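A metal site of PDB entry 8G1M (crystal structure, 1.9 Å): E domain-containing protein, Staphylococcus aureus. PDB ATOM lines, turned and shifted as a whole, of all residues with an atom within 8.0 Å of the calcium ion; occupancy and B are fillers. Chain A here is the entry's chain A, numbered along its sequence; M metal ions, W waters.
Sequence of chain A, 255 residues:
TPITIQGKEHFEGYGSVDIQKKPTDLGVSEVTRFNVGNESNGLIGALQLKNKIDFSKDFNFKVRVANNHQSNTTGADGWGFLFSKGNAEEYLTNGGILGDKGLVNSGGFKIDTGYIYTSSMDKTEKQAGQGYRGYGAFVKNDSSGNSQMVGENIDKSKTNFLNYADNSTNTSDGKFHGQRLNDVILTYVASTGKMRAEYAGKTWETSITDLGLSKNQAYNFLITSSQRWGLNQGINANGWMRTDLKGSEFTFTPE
N of Asp 112 sits at hydrogen-bond distance from O of Tyr 135. The side-chain carboxylate (OD2) of Asp 112 sits close to the side-chain amino group (NZ) of Lys 110 (2.8 Å). The backbone NH of Gly 114 is in hydrogen-bond range of the backbone carbonyl oxygen of Asp 77 (3.2 Å). The backbone NH (N) of Gly 114 lies close to the backbone carbonyl oxygen (O) of Ala 76 (3.4 Å). The side-chain hydroxyl (OH) of Tyr 135 sits close to the side-chain carboxylate (OD1) of Asp 122 (2.7 Å). The side-chain carboxylate of Asp 122 sits close to the backbone NH of Ile 116, at 2.7 Å. The backbone NH of Asp 122 sits at hydrogen-bond distance from the side-chain hydroxyl of Ser 119. The backbone carbonyl oxygen (O) of Gln 127 lies within hydrogen-bond range of the side-chain amide nitrogen (ND2) of Asn 72 (2.8 Å).
Within 4 Å of the calcium ion: Asp 112, Gly 114, Asp 122 and Gln 127. The nearest printed residue that does not touch the calcium ion is Tyr 135 (4.3 Å).
The calcium ion is bound by the side-chain carboxylate (OD1) of Asp 112, the side-chain carboxylate (OD2) of Asp 112, the backbone carbonyl oxygen (O) of Gly 114, water W2, the side-chain carboxylate (OD1) of Asp 122, water W1, the side-chain carboxylate (OD2) of Asp 122 and the side-chain amide oxygen (OE1) of Gln 127.
Water W2 lies within hydrogen-bond range of O of Asp 77 (2.9 Å) and O of Leu 98 (2.9 Å).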
ATOM      1  N   ASN A  72       2.605  -4.156 -19.515  1.00  0.00           N
ATOM      2  CA  ASN A  72       3.203  -4.949 -20.586  1.00  0.00           C
ATOM      3  C   ASN A  72       2.289  -5.106 -21.794  1.00  0.00           C
ATOM      4  O   ASN A  72       2.696  -5.710 -22.794  1.00  0.00           O
ATOM      5  CB  ASN A  72       3.662  -6.333 -20.057  1.00  0.00           C
ATOM      6  CG  ASN A  72       2.516  -7.313 -19.772  1.00  0.00           C
ATOM      7  OD1 ASN A  72       1.352  -7.026 -19.965  1.00  0.00           O
ATOM      8  ND2 ASN A  72       2.879  -8.511 -19.298  1.00  0.00           N
ATOM      9  N   ALA A  76       6.990  -1.273 -23.872  1.00  0.00           N
ATOM     10  CA  ALA A  76       7.952  -1.767 -24.842  1.00  0.00           C
ATOM     11  C   ALA A  76       7.918  -3.294 -24.920  1.00  0.00           C
ATOM     12  O   ALA A  76       7.511  -3.980 -23.967  1.00  0.00           O
ATOM     13  CB  ALA A  76       9.368  -1.311 -24.494  1.00  0.00           C
ATOM     14  N   ASP A  77       8.377  -3.822 -26.057  1.00  0.00           N
ATOM     15  CA  ASP A  77       8.429  -5.264 -26.249  1.00  0.00           C
ATOM     16  C   ASP A  77       9.553  -5.919 -25.448  1.00  0.00           C
ATOM     17  O   ASP A  77       9.444  -7.092 -25.051  1.00  0.00           O
ATOM     18  CB  ASP A  77       8.598  -5.578 -27.736  1.00  0.00           C
ATOM     19  CG  ASP A  77       7.478  -4.983 -28.581  1.00  0.00           C
ATOM     20  OD1 ASP A  77       6.417  -4.667 -28.009  1.00  0.00           O
ATOM     21  OD2 ASP A  77       7.664  -4.834 -29.818  1.00  0.00           O
ATOM     22  N   GLY A  78      10.659  -5.205 -25.238  1.00  0.00           N
ATOM     23  CA  GLY A  78      11.755  -5.675 -24.413  1.00  0.00           C
ATOM     24  C   GLY A  78      13.102  -5.258 -24.998  1.00  0.00           C
ATOM     25  O   GLY A  78      13.194  -4.303 -25.768  1.00  0.00           O
ATOM     26  N   ILE A  97      14.345 -10.432 -32.329  1.00  0.00           N
ATOM     27  CA  ILE A  97      14.030 -11.602 -31.529  1.00  0.00           C
ATOM     28  C   ILE A  97      13.009 -11.296 -30.430  1.00  0.00           C
ATOM     29  O   ILE A  97      12.889 -12.057 -29.472  1.00  0.00           O
ATOM     30  CB  ILE A  97      15.302 -12.241 -30.926  1.00  0.00           C
ATOM     31  CG1 ILE A  97      16.095 -11.191 -30.126  1.00  0.00           C
ATOM     32  CG2 ILE A  97      16.134 -12.883 -32.006  1.00  0.00           C
ATOM     33  CD1 ILE A  97      17.378 -11.761 -29.453  1.00  0.00           C
ATOM     34  N   LEU A  98      12.262 -10.199 -30.539  1.00  0.00           N
ATOM     35  CA  LEU A  98      11.274  -9.874 -29.510  1.00  0.00           C
ATOM     36  C   LEU A  98       9.846 -10.268 -29.893  1.00  0.00           C
ATOM     37  O   LEU A  98       8.900  -9.941 -29.170  1.00  0.00           O
ATOM     38  CB  LEU A  98      11.348  -8.380 -29.160  1.00  0.00           C
ATOM     39  CG  LEU A  98      12.591  -8.050 -28.311  1.00  0.00           C
ATOM     40  CD1 LEU A  98      12.834  -6.553 -28.224  1.00  0.00           C
ATOM     41  CD2 LEU A  98      12.424  -8.644 -26.916  1.00  0.00           C
ATOM     42  N   GLY A  99       9.677 -10.999 -30.990  1.00  0.00           N
ATOM     43  CA  GLY A  99       8.350 -11.410 -31.390  1.00  0.00           C
ATOM     44  C   GLY A  99       8.306 -12.855 -31.864  1.00  0.00           C
ATOM     45  O   GLY A  99       8.982 -13.704 -31.303  1.00  0.00           O
ATOM     46  N   ASP A 100       7.509 -13.132 -32.907  1.00  0.00           N
ATOM     47  CA  ASP A 100       7.421 -14.466 -33.469  1.00  0.00           C
ATOM     48  C   ASP A 100       8.282 -14.643 -34.708  1.00  0.00           C
ATOM     49  O   ASP A 100       8.528 -15.801 -35.107  1.00  0.00           O
ATOM     50  CB  ASP A 100       5.970 -14.813 -33.811  1.00  0.00           C
ATOM     51  CG  ASP A 100       5.102 -14.997 -32.570  1.00  0.00           C
ATOM     52  OD1 ASP A 100       5.679 -15.255 -31.488  1.00  0.00           O
ATOM     53  OD2 ASP A 100       3.858 -14.889 -32.669  1.00  0.00           O
ATOM     54  N   LYS A 110      17.079 -12.242 -25.225  1.00  0.00           N
ATOM     55  CA  LYS A 110      16.044 -11.236 -25.053  1.00  0.00           C
ATOM     56  C   LYS A 110      15.665 -11.093 -23.586  1.00  0.00           C
ATOM     57  O   LYS A 110      15.689 -12.069 -22.812  1.00  0.00           O
ATOM     58  CB  LYS A 110      14.800 -11.578 -25.894  1.00  0.00           C
ATOM     59  CG  LYS A 110      13.869 -12.655 -25.299  1.00  0.00           C
ATOM     60  CD  LYS A 110      12.525 -12.629 -26.057  1.00  0.00           C
ATOM     61  CE  LYS A 110      11.670 -13.851 -25.812  1.00  0.00           C
ATOM     62  NZ  LYS A 110      10.311 -13.685 -26.405  1.00  0.00           N
ATOM     63  N   ILE A 111      15.358  -9.856 -23.197  1.00  0.00           N
ATOM     64  CA  ILE A 111      14.631  -9.533 -21.968  1.00  0.00           C
ATOM     65  C   ILE A 111      13.258  -9.095 -22.435  1.00  0.00           C
ATOM     66  O   ILE A 111      13.105  -8.005 -23.014  1.00  0.00           O
ATOM     67  CB  ILE A 111      15.328  -8.425 -21.157  1.00  0.00           C
ATOM     68  CG1 ILE A 111      16.787  -8.813 -20.827  1.00  0.00           C
ATOM     69  CG2 ILE A 111      14.562  -8.135 -19.841  1.00  0.00           C
ATOM     70  CD1 ILE A 111      17.618  -7.665 -20.251  1.00  0.00           C
ATOM     71  N   ASP A 112      12.265  -9.944 -22.240  1.00  0.00           N
ATOM     72  CA  ASP A 112      10.948  -9.751 -22.835  1.00  0.00           C
ATOM     73  C   ASP A 112      10.073  -9.044 -21.808  1.00  0.00           C
ATOM     74  O   ASP A 112       9.796  -9.592 -20.735  1.00  0.00           O
ATOM     75  CB  ASP A 112      10.357 -11.106 -23.250  1.00  0.00           C
ATOM     76  CG  ASP A 112       9.066 -10.976 -24.048  1.00  0.00           C
ATOM     77  OD1 ASP A 112       8.223 -10.112 -23.710  1.00  0.00           O
ATOM     78  OD2 ASP A 112       8.888 -11.742 -25.004  1.00  0.00           O
ATOM     79  N   THR A 113       9.620  -7.838 -22.151  1.00  0.00           N
ATOM     80  CA  THR A 113       8.836  -6.994 -21.251  1.00  0.00           C
ATOM     81  C   THR A 113       7.438  -6.695 -21.784  1.00  0.00           C
ATOM     82  O   THR A 113       6.688  -5.983 -21.109  1.00  0.00           O
ATOM     83  CB  THR A 113       9.571  -5.672 -20.992  1.00  0.00           C
ATOM     84  OG1 THR A 113       9.656  -4.920 -22.210  1.00  0.00           O
ATOM     85  CG2 THR A 113      10.981  -5.938 -20.428  1.00  0.00           C
ATOM     86  N   GLY A 114       7.080  -7.206 -22.957  1.00  0.00           N
ATOM     87  CA  GLY A 114       5.810  -6.851 -23.563  1.00  0.00           C
ATOM     88  C   GLY A 114       4.979  -8.051 -23.961  1.00  0.00           C
ATOM     89  O   GLY A 114       5.490  -8.989 -24.596  1.00  0.00           O
ATOM     90  N   TYR A 115       3.706  -8.059 -23.576  1.00  0.00           N
ATOM     91  CA  TYR A 115       2.836  -9.194 -23.827  1.00  0.00           C
ATOM     92  C   TYR A 115       2.224  -9.020 -25.197  1.00  0.00           C
ATOM     93  O   TYR A 115       1.485  -8.055 -25.434  1.00  0.00           O
ATOM     94  CB  TYR A 115       1.745  -9.293 -22.757  1.00  0.00           C
ATOM     95  CG  TYR A 115       0.754 -10.399 -23.012  1.00  0.00           C
ATOM     96  CD1 TYR A 115       1.184 -11.674 -23.375  1.00  0.00           C
ATOM     97  CD2 TYR A 115      -0.613 -10.180 -22.851  1.00  0.00           C
ATOM     98  CE1 TYR A 115       0.265 -12.696 -23.591  1.00  0.00           C
ATOM     99  CE2 TYR A 115      -1.539 -11.195 -23.082  1.00  0.00           C
ATOM    100  CZ  TYR A 115      -1.089 -12.445 -23.436  1.00  0.00           C
ATOM    101  OH  TYR A 115      -1.996 -13.460 -23.654  1.00  0.00           O
ATOM    102  N   ILE A 116       2.526  -9.949 -26.095  1.00  0.00           N
ATOM    103  CA  ILE A 116       1.948  -9.978 -27.430  1.00  0.00           C
ATOM    104  C   ILE A 116       0.975 -11.145 -27.436  1.00  0.00           C
ATOM    105  O   ILE A 116       1.375 -12.300 -27.602  1.00  0.00           O
ATOM    106  CB  ILE A 116       3.027 -10.103 -28.515  1.00  0.00           C
ATOM    107  CG1 ILE A 116       3.962  -8.887 -28.453  1.00  0.00           C
ATOM    108  CG2 ILE A 116       2.381 -10.213 -29.896  1.00  0.00           C
ATOM    109  CD1 ILE A 116       5.179  -8.962 -29.359  1.00  0.00           C
ATOM    110  N   TYR A 117      -0.315 -10.852 -27.250  1.00  0.00           N
ATOM    111  CA  TYR A 117      -1.253 -11.881 -26.839  1.00  0.00           C
ATOM    112  C   TYR A 117      -1.471 -12.952 -27.904  1.00  0.00           C
ATOM    113  O   TYR A 117      -2.084 -13.980 -27.610  1.00  0.00           O
ATOM    114  CB  TYR A 117      -2.598 -11.280 -26.440  1.00  0.00           C
ATOM    115  CG  TYR A 117      -3.445 -10.735 -27.576  1.00  0.00           C
ATOM    116  CD1 TYR A 117      -3.211  -9.474 -28.098  1.00  0.00           C
ATOM    117  CD2 TYR A 117      -4.522 -11.467 -28.095  1.00  0.00           C
ATOM    118  CE1 TYR A 117      -3.989  -8.951 -29.124  1.00  0.00           C
ATOM    119  CE2 TYR A 117      -5.318 -10.956 -29.125  1.00  0.00           C
ATOM    120  CZ  TYR A 117      -5.037  -9.699 -29.630  1.00  0.00           C
ATOM    121  OH  TYR A 117      -5.801  -9.167 -30.645  1.00  0.00           O
ATOM    122  N   SER A 119       1.194 -14.372 -29.462  1.00  0.00           N
ATOM    123  CA  SER A 119       2.476 -15.062 -29.599  1.00  0.00           C
ATOM    124  C   SER A 119       2.529 -16.300 -28.705  1.00  0.00           C
ATOM    125  O   SER A 119       2.270 -16.211 -27.503  1.00  0.00           O
ATOM    126  CB  SER A 119       3.636 -14.129 -29.265  1.00  0.00           C
ATOM    127  OG  SER A 119       4.789 -14.831 -28.870  1.00  0.00           O
ATOM    128  N   MET A 121       5.142 -18.077 -27.648  1.00  0.00           N
ATOM    129  CA  MET A 121       6.156 -18.017 -26.596  1.00  0.00           C
ATOM    130  C   MET A 121       5.667 -17.207 -25.389  1.00  0.00           C
ATOM    131  O   MET A 121       5.864 -17.624 -24.244  1.00  0.00           O
ATOM    132  CB  MET A 121       7.463 -17.434 -27.147  1.00  0.00           C
ATOM    133  CG  MET A 121       8.688 -17.943 -26.403  1.00  0.00           C
ATOM    134  SD  MET A 121      10.184 -17.040 -26.806  1.00  0.00           S
ATOM    135  CE  MET A 121      10.156 -17.150 -28.604  1.00  0.00           C
ATOM    136  N   ASP A 122       4.999 -16.065 -25.642  1.00  0.00           N
ATOM    137  CA  ASP A 122       4.443 -15.256 -24.564  1.00  0.00           C
ATOM    138  C   ASP A 122       3.373 -16.021 -23.782  1.00  0.00           C
ATOM    139  O   ASP A 122       3.286 -15.904 -22.560  1.00  0.00           O
ATOM    140  CB  ASP A 122       3.850 -13.960 -25.109  1.00  0.00           C
ATOM    141  CG  ASP A 122       4.917 -12.941 -25.505  1.00  0.00           C
ATOM    142  OD1 ASP A 122       6.139 -13.257 -25.458  1.00  0.00           O
ATOM    143  OD2 ASP A 122       4.512 -11.814 -25.894  1.00  0.00           O
ATOM    144  N   LYS A 123       2.530 -16.790 -24.489  1.00  0.00           N
ATOM    145  CA  LYS A 123       1.481 -17.545 -23.789  1.00  0.00           C
ATOM    146  C   LYS A 123       2.074 -18.635 -22.910  1.00  0.00           C
ATOM    147  O   LYS A 123       1.682 -18.802 -21.748  1.00  0.00           O
ATOM    148  CB  LYS A 123       0.508 -18.149 -24.802  1.00  0.00           C
ATOM    149  CG  LYS A 123      -0.392 -17.154 -25.512  1.00  0.00           C
ATOM    150  CD  LYS A 123      -1.159 -17.913 -26.587  1.00  0.00           C
ATOM    151  CE  LYS A 123      -1.870 -16.998 -27.553  1.00  0.00           C
ATOM    152  NZ  LYS A 123      -2.281 -17.713 -28.796  1.00  0.00           N
ATOM    153  N   GLU A 125       4.901 -18.580 -21.552  1.00  0.00           N
ATOM    154  CA  GLU A 125       5.585 -17.956 -20.430  1.00  0.00           C
ATOM    155  C   GLU A 125       4.631 -17.244 -19.487  1.00  0.00           C
ATOM    156  O   GLU A 125       5.066 -16.586 -18.534  1.00  0.00           O
ATOM    157  CB  GLU A 125       6.659 -16.997 -20.942  1.00  0.00           C
ATOM    158  CG  GLU A 125       7.842 -17.724 -21.536  1.00  0.00           C
ATOM    159  CD  GLU A 125       8.592 -18.576 -20.510  1.00  0.00           C
ATOM    160  OE1 GLU A 125       8.696 -18.146 -19.341  1.00  0.00           O
ATOM    161  OE2 GLU A 125       9.078 -19.661 -20.881  1.00  0.00           O
ATOM    162  N   GLN A 127       2.844 -14.575 -19.779  1.00  0.00           N
ATOM    163  CA  GLN A 127       3.174 -13.164 -19.656  1.00  0.00           C
ATOM    164  C   GLN A 127       1.942 -12.282 -19.419  1.00  0.00           C
ATOM    165  O   GLN A 127       2.089 -11.207 -18.840  1.00  0.00           O
ATOM    166  CB  GLN A 127       3.927 -12.696 -20.904  1.00  0.00           C
ATOM    167  CG  GLN A 127       4.464 -11.272 -20.806  1.00  0.00           C
ATOM    168  CD  GLN A 127       5.540 -10.967 -21.849  1.00  0.00           C
ATOM    169  OE1 GLN A 127       5.536 -11.531 -22.942  1.00  0.00           O
ATOM    170  NE2 GLN A 127       6.453 -10.063 -21.518  1.00  0.00           N
ATOM    171  N   ARG A 133       5.092  -8.316 -15.806  1.00  0.00           N
ATOM    172  CA  ARG A 133       5.433  -9.705 -16.081  1.00  0.00           C
ATOM    173  C   ARG A 133       6.285  -9.795 -17.344  1.00  0.00           C
ATOM    174  O   ARG A 133       5.849  -9.398 -18.424  1.00  0.00           O
ATOM    175  CB  ARG A 133       4.173 -10.565 -16.255  1.00  0.00           C
ATOM    176  CG  ARG A 133       3.266 -10.608 -15.013  1.00  0.00           C
ATOM    177  CD  ARG A 133       2.081 -11.538 -15.201  1.00  0.00           C
ATOM    178  NE  ARG A 133       2.516 -12.902 -15.483  1.00  0.00           N
ATOM    179  CZ  ARG A 133       3.085 -13.711 -14.592  1.00  0.00           C
ATOM    180  NH1 ARG A 133       3.276 -13.304 -13.351  1.00  0.00           N
ATOM    181  NH2 ARG A 133       3.465 -14.935 -14.955  1.00  0.00           N
ATOM    182  N   GLY A 134       7.487 -10.357 -17.201  1.00  0.00           N
ATOM    183  CA  GLY A 134       8.398 -10.532 -18.311  1.00  0.00           C
ATOM    184  C   GLY A 134       9.159 -11.834 -18.193  1.00  0.00           C
ATOM    185  O   GLY A 134       8.846 -12.654 -17.327  1.00  0.00           O
ATOM    186  N   TYR A 135      10.169 -12.028 -19.025  1.00  0.00           N
ATOM    187  CA  TYR A 135      10.982 -13.239 -18.952  1.00  0.00           C
ATOM    188  C   TYR A 135      12.217 -13.039 -19.822  1.00  0.00           C
ATOM    189  O   TYR A 135      12.212 -12.212 -20.723  1.00  0.00           O
ATOM    190  CB  TYR A 135      10.200 -14.492 -19.400  1.00  0.00           C
ATOM    191  CG  TYR A 135       9.692 -14.540 -20.834  1.00  0.00           C
ATOM    192  CD1 TYR A 135       8.485 -13.942 -21.189  1.00  0.00           C
ATOM    193  CD2 TYR A 135      10.391 -15.240 -21.820  1.00  0.00           C
ATOM    194  CE1 TYR A 135       7.996 -14.019 -22.485  1.00  0.00           C
ATOM    195  CE2 TYR A 135       9.920 -15.329 -23.110  1.00  0.00           C
ATOM    196  CZ  TYR A 135       8.722 -14.725 -23.445  1.00  0.00           C
ATOM    197  OH  TYR A 135       8.271 -14.825 -24.750  1.00  0.00           O
ATOM    198  N   ARG A 228       5.337  -2.468 -29.323  1.00  0.00           N
ATOM    199  CA  ARG A 228       4.153  -2.887 -30.067  1.00  0.00           C
ATOM    200  C   ARG A 228       4.415  -2.939 -31.575  1.00  0.00           C
ATOM    201  O   ARG A 228       3.495  -2.737 -32.375  1.00  0.00           O
ATOM    202  CB  ARG A 228       2.971  -1.958 -29.769  1.00  0.00           C
ATOM    203  CG  ARG A 228       2.731  -1.629 -28.283  1.00  0.00           C
ATOM    204  CD  ARG A 228       2.686  -2.896 -27.424  1.00  0.00           C
ATOM    205  NE  ARG A 228       1.511  -3.704 -27.686  1.00  0.00           N
ATOM    206  CZ  ARG A 228       1.293  -4.906 -27.158  1.00  0.00           C
ATOM    207  NH1 ARG A 228       0.175  -5.571 -27.444  1.00  0.00           N
ATOM    208  NH2 ARG A 228       2.187  -5.447 -26.337  1.00  0.00           N
HETATM  209 CA    CA M   1       6.739 -10.872 -25.332  1.00  0.00          CA
HETATM  210  O   HOH W   1       7.017 -11.454 -27.725  1.00  0.00           O
HETATM  211  O   HOH W   2       7.985  -9.115 -26.497  1.00  0.00           O
